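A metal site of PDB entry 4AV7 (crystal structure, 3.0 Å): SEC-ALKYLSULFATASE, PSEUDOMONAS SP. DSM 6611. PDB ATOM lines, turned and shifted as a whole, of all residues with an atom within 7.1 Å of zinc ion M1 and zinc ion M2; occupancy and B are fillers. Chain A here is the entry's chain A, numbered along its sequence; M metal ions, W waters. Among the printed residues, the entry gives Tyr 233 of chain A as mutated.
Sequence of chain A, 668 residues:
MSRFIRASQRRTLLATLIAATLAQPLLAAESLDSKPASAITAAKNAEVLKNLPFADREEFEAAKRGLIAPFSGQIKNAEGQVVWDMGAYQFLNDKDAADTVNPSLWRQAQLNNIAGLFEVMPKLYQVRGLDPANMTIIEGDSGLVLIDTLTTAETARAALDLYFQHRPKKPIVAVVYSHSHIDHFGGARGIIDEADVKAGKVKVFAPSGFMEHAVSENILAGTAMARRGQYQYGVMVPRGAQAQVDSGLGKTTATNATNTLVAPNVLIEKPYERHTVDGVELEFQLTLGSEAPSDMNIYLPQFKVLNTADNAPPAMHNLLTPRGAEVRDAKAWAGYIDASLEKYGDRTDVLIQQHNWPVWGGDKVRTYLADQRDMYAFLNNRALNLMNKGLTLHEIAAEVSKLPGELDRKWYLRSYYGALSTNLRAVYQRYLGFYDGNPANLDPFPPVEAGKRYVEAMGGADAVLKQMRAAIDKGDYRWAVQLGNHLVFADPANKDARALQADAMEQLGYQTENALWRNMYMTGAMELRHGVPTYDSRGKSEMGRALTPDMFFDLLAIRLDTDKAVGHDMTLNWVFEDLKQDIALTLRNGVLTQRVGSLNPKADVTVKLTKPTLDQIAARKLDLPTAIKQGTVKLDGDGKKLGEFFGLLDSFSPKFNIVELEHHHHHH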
ATOM      1  N   PRO A 132     -23.007 -16.664  -1.622  1.00  0.00           N
ATOM      2  CA  PRO A 132     -22.061 -17.610  -2.238  1.00  0.00           C
ATOM      3  C   PRO A 132     -21.707 -17.246  -3.684  1.00  0.00           C
ATOM      4  O   PRO A 132     -20.565 -17.449  -4.081  1.00  0.00           O
ATOM      5  CB  PRO A 132     -22.805 -18.939  -2.211  1.00  0.00           C
ATOM      6  CG  PRO A 132     -24.197 -18.642  -1.714  1.00  0.00           C
ATOM      7  CD  PRO A 132     -24.114 -17.355  -0.954  1.00  0.00           C
ATOM      8  N   ALA A 133     -22.661 -16.705  -4.440  1.00  0.00           N
ATOM      9  CA  ALA A 133     -22.466 -16.312  -5.846  1.00  0.00           C
ATOM     10  C   ALA A 133     -22.148 -14.818  -6.061  1.00  0.00           C
ATOM     11  O   ALA A 133     -22.019 -14.054  -5.112  1.00  0.00           O
ATOM     12  CB  ALA A 133     -23.688 -16.711  -6.652  1.00  0.00           C
ATOM     13  N   ASN A 134     -22.040 -14.407  -7.315  1.00  0.00           N
ATOM     14  CA  ASN A 134     -21.881 -12.991  -7.631  1.00  0.00           C
ATOM     15  C   ASN A 134     -23.095 -12.369  -8.372  1.00  0.00           C
ATOM     16  O   ASN A 134     -23.979 -13.072  -8.923  1.00  0.00           O
ATOM     17  CB  ASN A 134     -20.591 -12.783  -8.425  1.00  0.00           C
ATOM     18  CG  ASN A 134     -19.328 -13.164  -7.654  1.00  0.00           C
ATOM     19  OD1 ASN A 134     -19.350 -13.360  -6.416  1.00  0.00           O
ATOM     20  ND2 ASN A 134     -18.201 -13.267  -8.378  1.00  0.00           N
ATOM     21  N   ASP A 148     -27.754 -12.695 -13.022  1.00  0.00           N
ATOM     22  CA  ASP A 148     -27.965 -13.448 -11.774  1.00  0.00           C
ATOM     23  C   ASP A 148     -28.354 -12.565 -10.602  1.00  0.00           C
ATOM     24  O   ASP A 148     -27.897 -11.432 -10.487  1.00  0.00           O
ATOM     25  CB  ASP A 148     -26.781 -14.333 -11.429  1.00  0.00           C
ATOM     26  CG  ASP A 148     -26.524 -15.378 -12.487  1.00  0.00           C
ATOM     27  OD1 ASP A 148     -27.501 -15.765 -13.177  1.00  0.00           O
ATOM     28  OD2 ASP A 148     -25.359 -15.811 -12.640  1.00  0.00           O
ATOM     29  N   SER A 178     -28.126 -17.029 -15.671  1.00  0.00           N
ATOM     30  CA  SER A 178     -27.076 -17.700 -16.407  1.00  0.00           C
ATOM     31  C   SER A 178     -27.204 -19.246 -16.377  1.00  0.00           C
ATOM     32  O   SER A 178     -26.722 -19.932 -17.295  1.00  0.00           O
ATOM     33  CB  SER A 178     -25.737 -17.281 -15.841  1.00  0.00           C
ATOM     34  OG  SER A 178     -25.659 -17.712 -14.496  1.00  0.00           O
ATOM     35  N   HIS A 179     -27.876 -19.773 -15.345  1.00  0.00           N
ATOM     36  CA  HIS A 179     -28.168 -21.208 -15.255  1.00  0.00           C
ATOM     37  C   HIS A 179     -29.191 -21.564 -14.193  1.00  0.00           C
ATOM     38  O   HIS A 179     -29.591 -20.708 -13.419  1.00  0.00           O
ATOM     39  CB  HIS A 179     -26.897 -22.043 -15.068  1.00  0.00           C
ATOM     40  CG  HIS A 179     -26.063 -21.680 -13.850  1.00  0.00           C
ATOM     41  ND1 HIS A 179     -25.263 -20.619 -13.805  1.00  0.00           N
ATOM     42  CD2 HIS A 179     -25.901 -22.343 -12.633  1.00  0.00           C
ATOM     43  CE1 HIS A 179     -24.626 -20.588 -12.620  1.00  0.00           C
ATOM     44  NE2 HIS A 179     -25.023 -21.647 -11.910  1.00  0.00           N
ATOM     45  N   SER A 180     -29.601 -22.830 -14.129  1.00  0.00           N
ATOM     46  CA  SER A 180     -30.696 -23.215 -13.238  1.00  0.00           C
ATOM     47  C   SER A 180     -30.195 -23.610 -11.858  1.00  0.00           C
ATOM     48  O   SER A 180     -30.616 -24.642 -11.319  1.00  0.00           O
ATOM     49  CB  SER A 180     -31.538 -24.340 -13.836  1.00  0.00           C
ATOM     50  OG  SER A 180     -30.722 -25.455 -14.153  1.00  0.00           O
ATOM     51  N   HIS A 181     -29.315 -22.790 -11.284  1.00  0.00           N
ATOM     52  CA  HIS A 181     -28.864 -22.981  -9.901  1.00  0.00           C
ATOM     53  C   HIS A 181     -29.357 -21.923  -8.948  1.00  0.00           C
ATOM     54  O   HIS A 181     -29.208 -20.714  -9.194  1.00  0.00           O
ATOM     55  CB  HIS A 181     -27.337 -23.096  -9.788  1.00  0.00           C
ATOM     56  CG  HIS A 181     -26.763 -24.429 -10.248  1.00  0.00           C
ATOM     57  ND1 HIS A 181     -25.444 -24.585 -10.563  1.00  0.00           N
ATOM     58  CD2 HIS A 181     -27.363 -25.671 -10.450  1.00  0.00           C
ATOM     59  CE1 HIS A 181     -25.216 -25.849 -10.944  1.00  0.00           C
ATOM     60  NE2 HIS A 181     -26.395 -26.524 -10.881  1.00  0.00           N
ATOM     61  N   ILE A 182     -29.939 -22.376  -7.833  1.00  0.00           N
ATOM     62  CA  ILE A 182     -30.563 -21.523  -6.815  1.00  0.00           C
ATOM     63  C   ILE A 182     -29.728 -20.295  -6.388  1.00  0.00           C
ATOM     64  O   ILE A 182     -30.276 -19.241  -6.065  1.00  0.00           O
ATOM     65  CB  ILE A 182     -30.979 -22.380  -5.612  1.00  0.00           C
ATOM     66  CG1 ILE A 182     -32.193 -21.753  -4.910  1.00  0.00           C
ATOM     67  CG2 ILE A 182     -29.788 -22.583  -4.666  1.00  0.00           C
ATOM     68  CD1 ILE A 182     -32.844 -22.662  -3.902  1.00  0.00           C
ATOM     69  N   ASP A 183     -28.409 -20.409  -6.411  1.00  0.00           N
ATOM     70  CA  ASP A 183     -27.542 -19.294  -6.054  1.00  0.00           C
ATOM     71  C   ASP A 183     -27.507 -18.215  -7.137  1.00  0.00           C
ATOM     72  O   ASP A 183     -26.699 -17.273  -7.060  1.00  0.00           O
ATOM     73  CB  ASP A 183     -26.109 -19.785  -5.694  1.00  0.00           C
ATOM     74  CG  ASP A 183     -25.468 -20.696  -6.763  1.00  0.00           C
ATOM     75  OD1 ASP A 183     -26.183 -21.575  -7.299  1.00  0.00           O
ATOM     76  OD2 ASP A 183     -24.245 -20.572  -7.055  1.00  0.00           O
ATOM     77  N   HIS A 184     -28.361 -18.347  -8.159  1.00  0.00           N
ATOM     78  CA  HIS A 184     -28.365 -17.395  -9.258  1.00  0.00           C
ATOM     79  C   HIS A 184     -29.736 -16.882  -9.595  1.00  0.00           C
ATOM     80  O   HIS A 184     -29.850 -15.770 -10.161  1.00  0.00           O
ATOM     81  CB  HIS A 184     -27.680 -17.994 -10.469  1.00  0.00           C
ATOM     82  CG  HIS A 184     -26.286 -18.479 -10.192  1.00  0.00           C
ATOM     83  ND1 HIS A 184     -25.198 -17.742 -10.461  1.00  0.00           N
ATOM     84  CD2 HIS A 184     -25.819 -19.671  -9.653  1.00  0.00           C
ATOM     85  CE1 HIS A 184     -24.103 -18.423 -10.101  1.00  0.00           C
ATOM     86  NE2 HIS A 184     -24.487 -19.605  -9.612  1.00  0.00           N
ATOM     87  N   TYR A 233     -22.050 -27.003   2.456  1.00  0.00           N
ATOM     88  CA  TYR A 233     -21.633 -25.639   2.851  1.00  0.00           C
ATOM     89  C   TYR A 233     -21.359 -25.493   4.359  1.00  0.00           C
ATOM     90  O   TYR A 233     -21.086 -24.377   4.831  1.00  0.00           O
ATOM     91  CB  TYR A 233     -22.686 -24.624   2.424  1.00  0.00           C
ATOM     92  CG  TYR A 233     -22.948 -24.615   0.947  1.00  0.00           C
ATOM     93  CD1 TYR A 233     -22.146 -23.872   0.085  1.00  0.00           C
ATOM     94  CD2 TYR A 233     -24.016 -25.349   0.407  1.00  0.00           C
ATOM     95  CE1 TYR A 233     -22.392 -23.845  -1.271  1.00  0.00           C
ATOM     96  CE2 TYR A 233     -24.261 -25.339  -0.967  1.00  0.00           C
ATOM     97  CZ  TYR A 233     -23.449 -24.568  -1.793  1.00  0.00           C
ATOM     98  OH  TYR A 233     -23.646 -24.517  -3.151  1.00  0.00           O
ATOM     99  N   LEU A 249     -15.946 -21.759  -3.861  1.00  0.00           N
ATOM    100  CA  LEU A 249     -16.381 -20.721  -4.762  1.00  0.00           C
ATOM    101  C   LEU A 249     -17.157 -19.684  -3.994  1.00  0.00           C
ATOM    102  O   LEU A 249     -17.919 -18.889  -4.572  1.00  0.00           O
ATOM    103  CB  LEU A 249     -17.237 -21.295  -5.872  1.00  0.00           C
ATOM    104  CG  LEU A 249     -16.662 -22.462  -6.672  1.00  0.00           C
ATOM    105  CD1 LEU A 249     -17.652 -22.843  -7.758  1.00  0.00           C
ATOM    106  CD2 LEU A 249     -15.297 -22.141  -7.261  1.00  0.00           C
ATOM    107  N   GLU A 291     -22.091 -27.378 -16.520  1.00  0.00           N
ATOM    108  CA  GLU A 291     -22.158 -27.135 -15.064  1.00  0.00           C
ATOM    109  C   GLU A 291     -23.572 -27.306 -14.515  1.00  0.00           C
ATOM    110  O   GLU A 291     -23.753 -27.720 -13.368  1.00  0.00           O
ATOM    111  CB  GLU A 291     -21.632 -25.756 -14.704  1.00  0.00           C
ATOM    112  CG  GLU A 291     -21.521 -25.504 -13.191  1.00  0.00           C
ATOM    113  CD  GLU A 291     -22.590 -24.560 -12.605  1.00  0.00           C
ATOM    114  OE1 GLU A 291     -23.367 -23.895 -13.349  1.00  0.00           O
ATOM    115  OE2 GLU A 291     -22.636 -24.440 -11.358  1.00  0.00           O
ATOM    116  N   ALA A 292     -24.551 -26.991 -15.356  1.00  0.00           N
ATOM    117  CA  ALA A 292     -25.959 -27.054 -15.016  1.00  0.00           C
ATOM    118  C   ALA A 292     -26.675 -27.608 -16.250  1.00  0.00           C
ATOM    119  O   ALA A 292     -26.200 -27.385 -17.372  1.00  0.00           O
ATOM    120  CB  ALA A 292     -26.480 -25.674 -14.713  1.00  0.00           C
ATOM    121  N   ASP A 295     -28.049 -23.876 -18.836  1.00  0.00           N
ATOM    122  CA  ASP A 295     -26.832 -23.086 -18.569  1.00  0.00           C
ATOM    123  C   ASP A 295     -26.337 -22.397 -19.854  1.00  0.00           C
ATOM    124  O   ASP A 295     -26.483 -22.954 -20.955  1.00  0.00           O
ATOM    125  CB  ASP A 295     -25.766 -24.032 -17.968  1.00  0.00           C
ATOM    126  CG  ASP A 295     -24.418 -23.369 -17.721  1.00  0.00           C
ATOM    127  OD1 ASP A 295     -24.354 -22.273 -17.119  1.00  0.00           O
ATOM    128  OD2 ASP A 295     -23.396 -23.984 -18.101  1.00  0.00           O
ATOM    129  N   ALA A 309     -20.145 -17.442 -16.459  1.00  0.00           N
ATOM    130  CA  ALA A 309     -21.029 -17.884 -15.388  1.00  0.00           C
ATOM    131  C   ALA A 309     -20.335 -18.827 -14.366  1.00  0.00           C
ATOM    132  O   ALA A 309     -19.475 -18.378 -13.603  1.00  0.00           O
ATOM    133  CB  ALA A 309     -22.276 -18.520 -15.963  1.00  0.00           C
ATOM    134  N   ASP A 310     -20.689 -20.096 -14.357  1.00  0.00           N
ATOM    135  CA  ASP A 310     -20.052 -21.081 -13.476  1.00  0.00           C
ATOM    136  C   ASP A 310     -19.253 -22.138 -14.258  1.00  0.00           C
ATOM    137  O   ASP A 310     -18.743 -23.084 -13.676  1.00  0.00           O
ATOM    138  CB  ASP A 310     -21.091 -21.777 -12.563  1.00  0.00           C
ATOM    139  CG  ASP A 310     -21.640 -20.865 -11.472  1.00  0.00           C
ATOM    140  OD1 ASP A 310     -21.432 -19.621 -11.547  1.00  0.00           O
ATOM    141  OD2 ASP A 310     -22.294 -21.401 -10.538  1.00  0.00           O
ATOM    142  N   ASN A 311     -19.097 -21.944 -15.553  1.00  0.00           N
ATOM    143  CA  ASN A 311     -18.389 -22.896 -16.370  1.00  0.00           C
ATOM    144  C   ASN A 311     -16.872 -22.927 -16.248  1.00  0.00           C
ATOM    145  O   ASN A 311     -16.249 -23.922 -16.617  1.00  0.00           O
ATOM    146  CB  ASN A 311     -18.811 -22.718 -17.817  1.00  0.00           C
ATOM    147  CG  ASN A 311     -20.315 -22.805 -17.983  1.00  0.00           C
ATOM    148  OD1 ASN A 311     -21.004 -23.380 -17.127  1.00  0.00           O
ATOM    149  ND2 ASN A 311     -20.831 -22.222 -19.050  1.00  0.00           N
ATOM    150  N   HIS A 317     -14.438 -27.616 -10.624  1.00  0.00           N
ATOM    151  CA  HIS A 317     -15.869 -27.638 -10.263  1.00  0.00           C
ATOM    152  C   HIS A 317     -16.317 -29.085 -10.104  1.00  0.00           C
ATOM    153  O   HIS A 317     -15.579 -29.991 -10.444  1.00  0.00           O
ATOM    154  CB  HIS A 317     -16.699 -26.885 -11.281  1.00  0.00           C
ATOM    155  CG  HIS A 317     -18.003 -26.293 -10.757  1.00  0.00           C
ATOM    156  ND1 HIS A 317     -18.779 -26.901  -9.847  1.00  0.00           N
ATOM    157  CD2 HIS A 317     -18.670 -25.129 -11.123  1.00  0.00           C
ATOM    158  CE1 HIS A 317     -19.868 -26.159  -9.620  1.00  0.00           C
ATOM    159  NE2 HIS A 317     -19.801 -25.071 -10.407  1.00  0.00           N
ATOM    160  N   ARG A 323     -24.526 -31.869  -2.578  1.00  0.00           N
ATOM    161  CA  ARG A 323     -25.919 -31.678  -2.189  1.00  0.00           C
ATOM    162  C   ARG A 323     -26.811 -32.626  -2.971  1.00  0.00           C
ATOM    163  O   ARG A 323     -27.911 -32.957  -2.511  1.00  0.00           O
ATOM    164  CB  ARG A 323     -26.339 -30.231  -2.431  1.00  0.00           C
ATOM    165  CG  ARG A 323     -26.439 -29.851  -3.910  1.00  0.00           C
ATOM    166  CD  ARG A 323     -26.511 -28.358  -4.073  1.00  0.00           C
ATOM    167  NE  ARG A 323     -26.138 -27.956  -5.423  1.00  0.00           N
ATOM    168  CZ  ARG A 323     -26.994 -27.824  -6.418  1.00  0.00           C
ATOM    169  NH1 ARG A 323     -28.284 -28.062  -6.230  1.00  0.00           N
ATOM    170  NH2 ARG A 323     -26.564 -27.429  -7.614  1.00  0.00           N
ATOM    171  N   ARG A 328     -22.896 -34.351 -14.460  1.00  0.00           N
ATOM    172  CA  ARG A 328     -22.509 -33.389 -15.442  1.00  0.00           C
ATOM    173  C   ARG A 328     -21.592 -33.967 -16.512  1.00  0.00           C
ATOM    174  O   ARG A 328     -20.805 -34.873 -16.258  1.00  0.00           O
ATOM    175  CB  ARG A 328     -21.876 -32.227 -14.713  1.00  0.00           C
ATOM    176  CG  ARG A 328     -22.935 -31.544 -13.875  1.00  0.00           C
ATOM    177  CD  ARG A 328     -22.332 -30.625 -12.865  1.00  0.00           C
ATOM    178  NE  ARG A 328     -23.393 -30.059 -12.063  1.00  0.00           N
ATOM    179  CZ  ARG A 328     -23.201 -29.471 -10.872  1.00  0.00           C
ATOM    180  NH1 ARG A 328     -21.989 -29.400 -10.330  1.00  0.00           N
ATOM    181  NH2 ARG A 328     -24.231 -28.962 -10.218  1.00  0.00           N
ATOM    182  N   GLN A 354     -19.497 -15.771 -12.301  1.00  0.00           N
ATOM    183  CA  GLN A 354     -20.556 -15.619 -11.322  1.00  0.00           C
ATOM    184  C   GLN A 354     -20.187 -16.132  -9.898  1.00  0.00           C
ATOM    185  O   GLN A 354     -21.027 -16.194  -8.974  1.00  0.00           O
ATOM    186  CB  GLN A 354     -21.843 -16.200 -11.874  1.00  0.00           C
ATOM    187  CG  GLN A 354     -22.439 -15.350 -13.008  1.00  0.00           C
ATOM    188  CD  GLN A 354     -22.562 -13.853 -12.676  1.00  0.00           C
ATOM    189  OE1 GLN A 354     -21.865 -13.029 -13.277  1.00  0.00           O
ATOM    190  NE2 GLN A 354     -23.462 -13.500 -11.745  1.00  0.00           N
ATOM    191  N   HIS A 355     -18.913 -16.503  -9.737  1.00  0.00           N
ATOM    192  CA  HIS A 355     -18.315 -16.921  -8.475  1.00  0.00           C
ATOM    193  C   HIS A 355     -16.895 -16.467  -8.613  1.00  0.00           C
ATOM    194  O   HIS A 355     -16.350 -16.438  -9.740  1.00  0.00           O
ATOM    195  CB  HIS A 355     -18.315 -18.434  -8.281  1.00  0.00           C
ATOM    196  CG  HIS A 355     -19.642 -19.032  -7.892  1.00  0.00           C
ATOM    197  ND1 HIS A 355     -20.069 -19.071  -6.621  1.00  0.00           N
ATOM    198  CD2 HIS A 355     -20.621 -19.681  -8.663  1.00  0.00           C
ATOM    199  CE1 HIS A 355     -21.275 -19.686  -6.573  1.00  0.00           C
ATOM    200  NE2 HIS A 355     -21.608 -20.056  -7.832  1.00  0.00           N
ATOM    201  N   TYR A 417     -13.264 -26.823  -4.788  1.00  0.00           N
ATOM    202  CA  TYR A 417     -14.706 -27.064  -4.911  1.00  0.00           C
ATOM    203  C   TYR A 417     -14.980 -28.528  -5.324  1.00  0.00           C
ATOM    204  O   TYR A 417     -15.349 -29.381  -4.493  1.00  0.00           O
ATOM    205  CB  TYR A 417     -15.334 -26.076  -5.910  1.00  0.00           C
ATOM    206  CG  TYR A 417     -16.794 -25.805  -5.627  1.00  0.00           C
ATOM    207  CD1 TYR A 417     -17.182 -25.084  -4.485  1.00  0.00           C
ATOM    208  CD2 TYR A 417     -17.795 -26.269  -6.484  1.00  0.00           C
ATOM    209  CE1 TYR A 417     -18.510 -24.829  -4.210  1.00  0.00           C
ATOM    210  CE2 TYR A 417     -19.127 -26.026  -6.215  1.00  0.00           C
ATOM    211  CZ  TYR A 417     -19.482 -25.301  -5.075  1.00  0.00           C
ATOM    212  OH  TYR A 417     -20.803 -25.047  -4.788  1.00  0.00           O
HETATM  213 ZN    ZN M   1     -23.871 -23.109 -10.723  1.00  0.00          ZN
HETATM  214 ZN    ZN M   2     -23.187 -20.799  -8.802  1.00  0.00          ZN
HETATM  215  O   HOH W   1     -24.179 -23.282  -7.892  1.00  0.00           O
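NE2 of His 181 is in hydrogen-bond range of NH2 of Arg 328 (3.3 Å). The side-chain carboxylate of Asp 148 sits at hydrogen-bond distance from a ring nitrogen (ND1) of His 184 (2.9 Å). ND1 of His 355 is in hydrogen-bond range of O of Leu 249. The side-chain hydroxyl (OG) of Ser 178 lies within hydrogen-bond range of a ring nitrogen (ND1) of His 179 (3.0 Å). The guanidinium group of Arg 328 lies within hydrogen-bond range of the backbone carbonyl oxygen of Glu 291 (2.7 Å). The side-chain carboxylate (OE2) of Glu 291 sits close to a ring nitrogen (NE2) of His 317 (3.1 Å). A ring nitrogen (ND1) of His 355 is in hydrogen-bond range of the backbone carbonyl oxygen (O) of Pro 132, 3.1 Å away. The guanidinium group (NH2) of Arg 323 sits at hydrogen-bond distance from a ring nitrogen (NE2) of His 181.
The nearest printed residue that does not touch zinc ion M2 is Glu 291 (4.5 Å).
Zinc ion M1 is bound by OE2 of Glu 291 (1.9 Å). Zinc ion M1 is bound by ND1 of His 181, 2.2 Å away. A ring nitrogen (NE2) of His 179 is bound to zinc ion M1 (2.2 Å). OD2 of Asp 310 binds zinc ion M1 (2.3 Å). Zinc ion M1 has four donor atoms within binding distance. Slightly farther from zinc ion M1 lies OE1 of Glu 291 (2.8 Å).
Zinc ion M2 is bound by NE2 of His 184 (1.9 Å). NE2 of His 355 binds zinc ion M2 (2.0 Å). OD2 of Asp 310 is bound to zinc ion M2, at 2.0 Å. The side-chain carboxylate (OD2) of Asp 183 binds zinc ion M2 (2.1 Å). Zinc ion M2 has four donor atoms within binding distance. Slightly farther from zinc ion M2 lies water W1 (2.8 Å).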
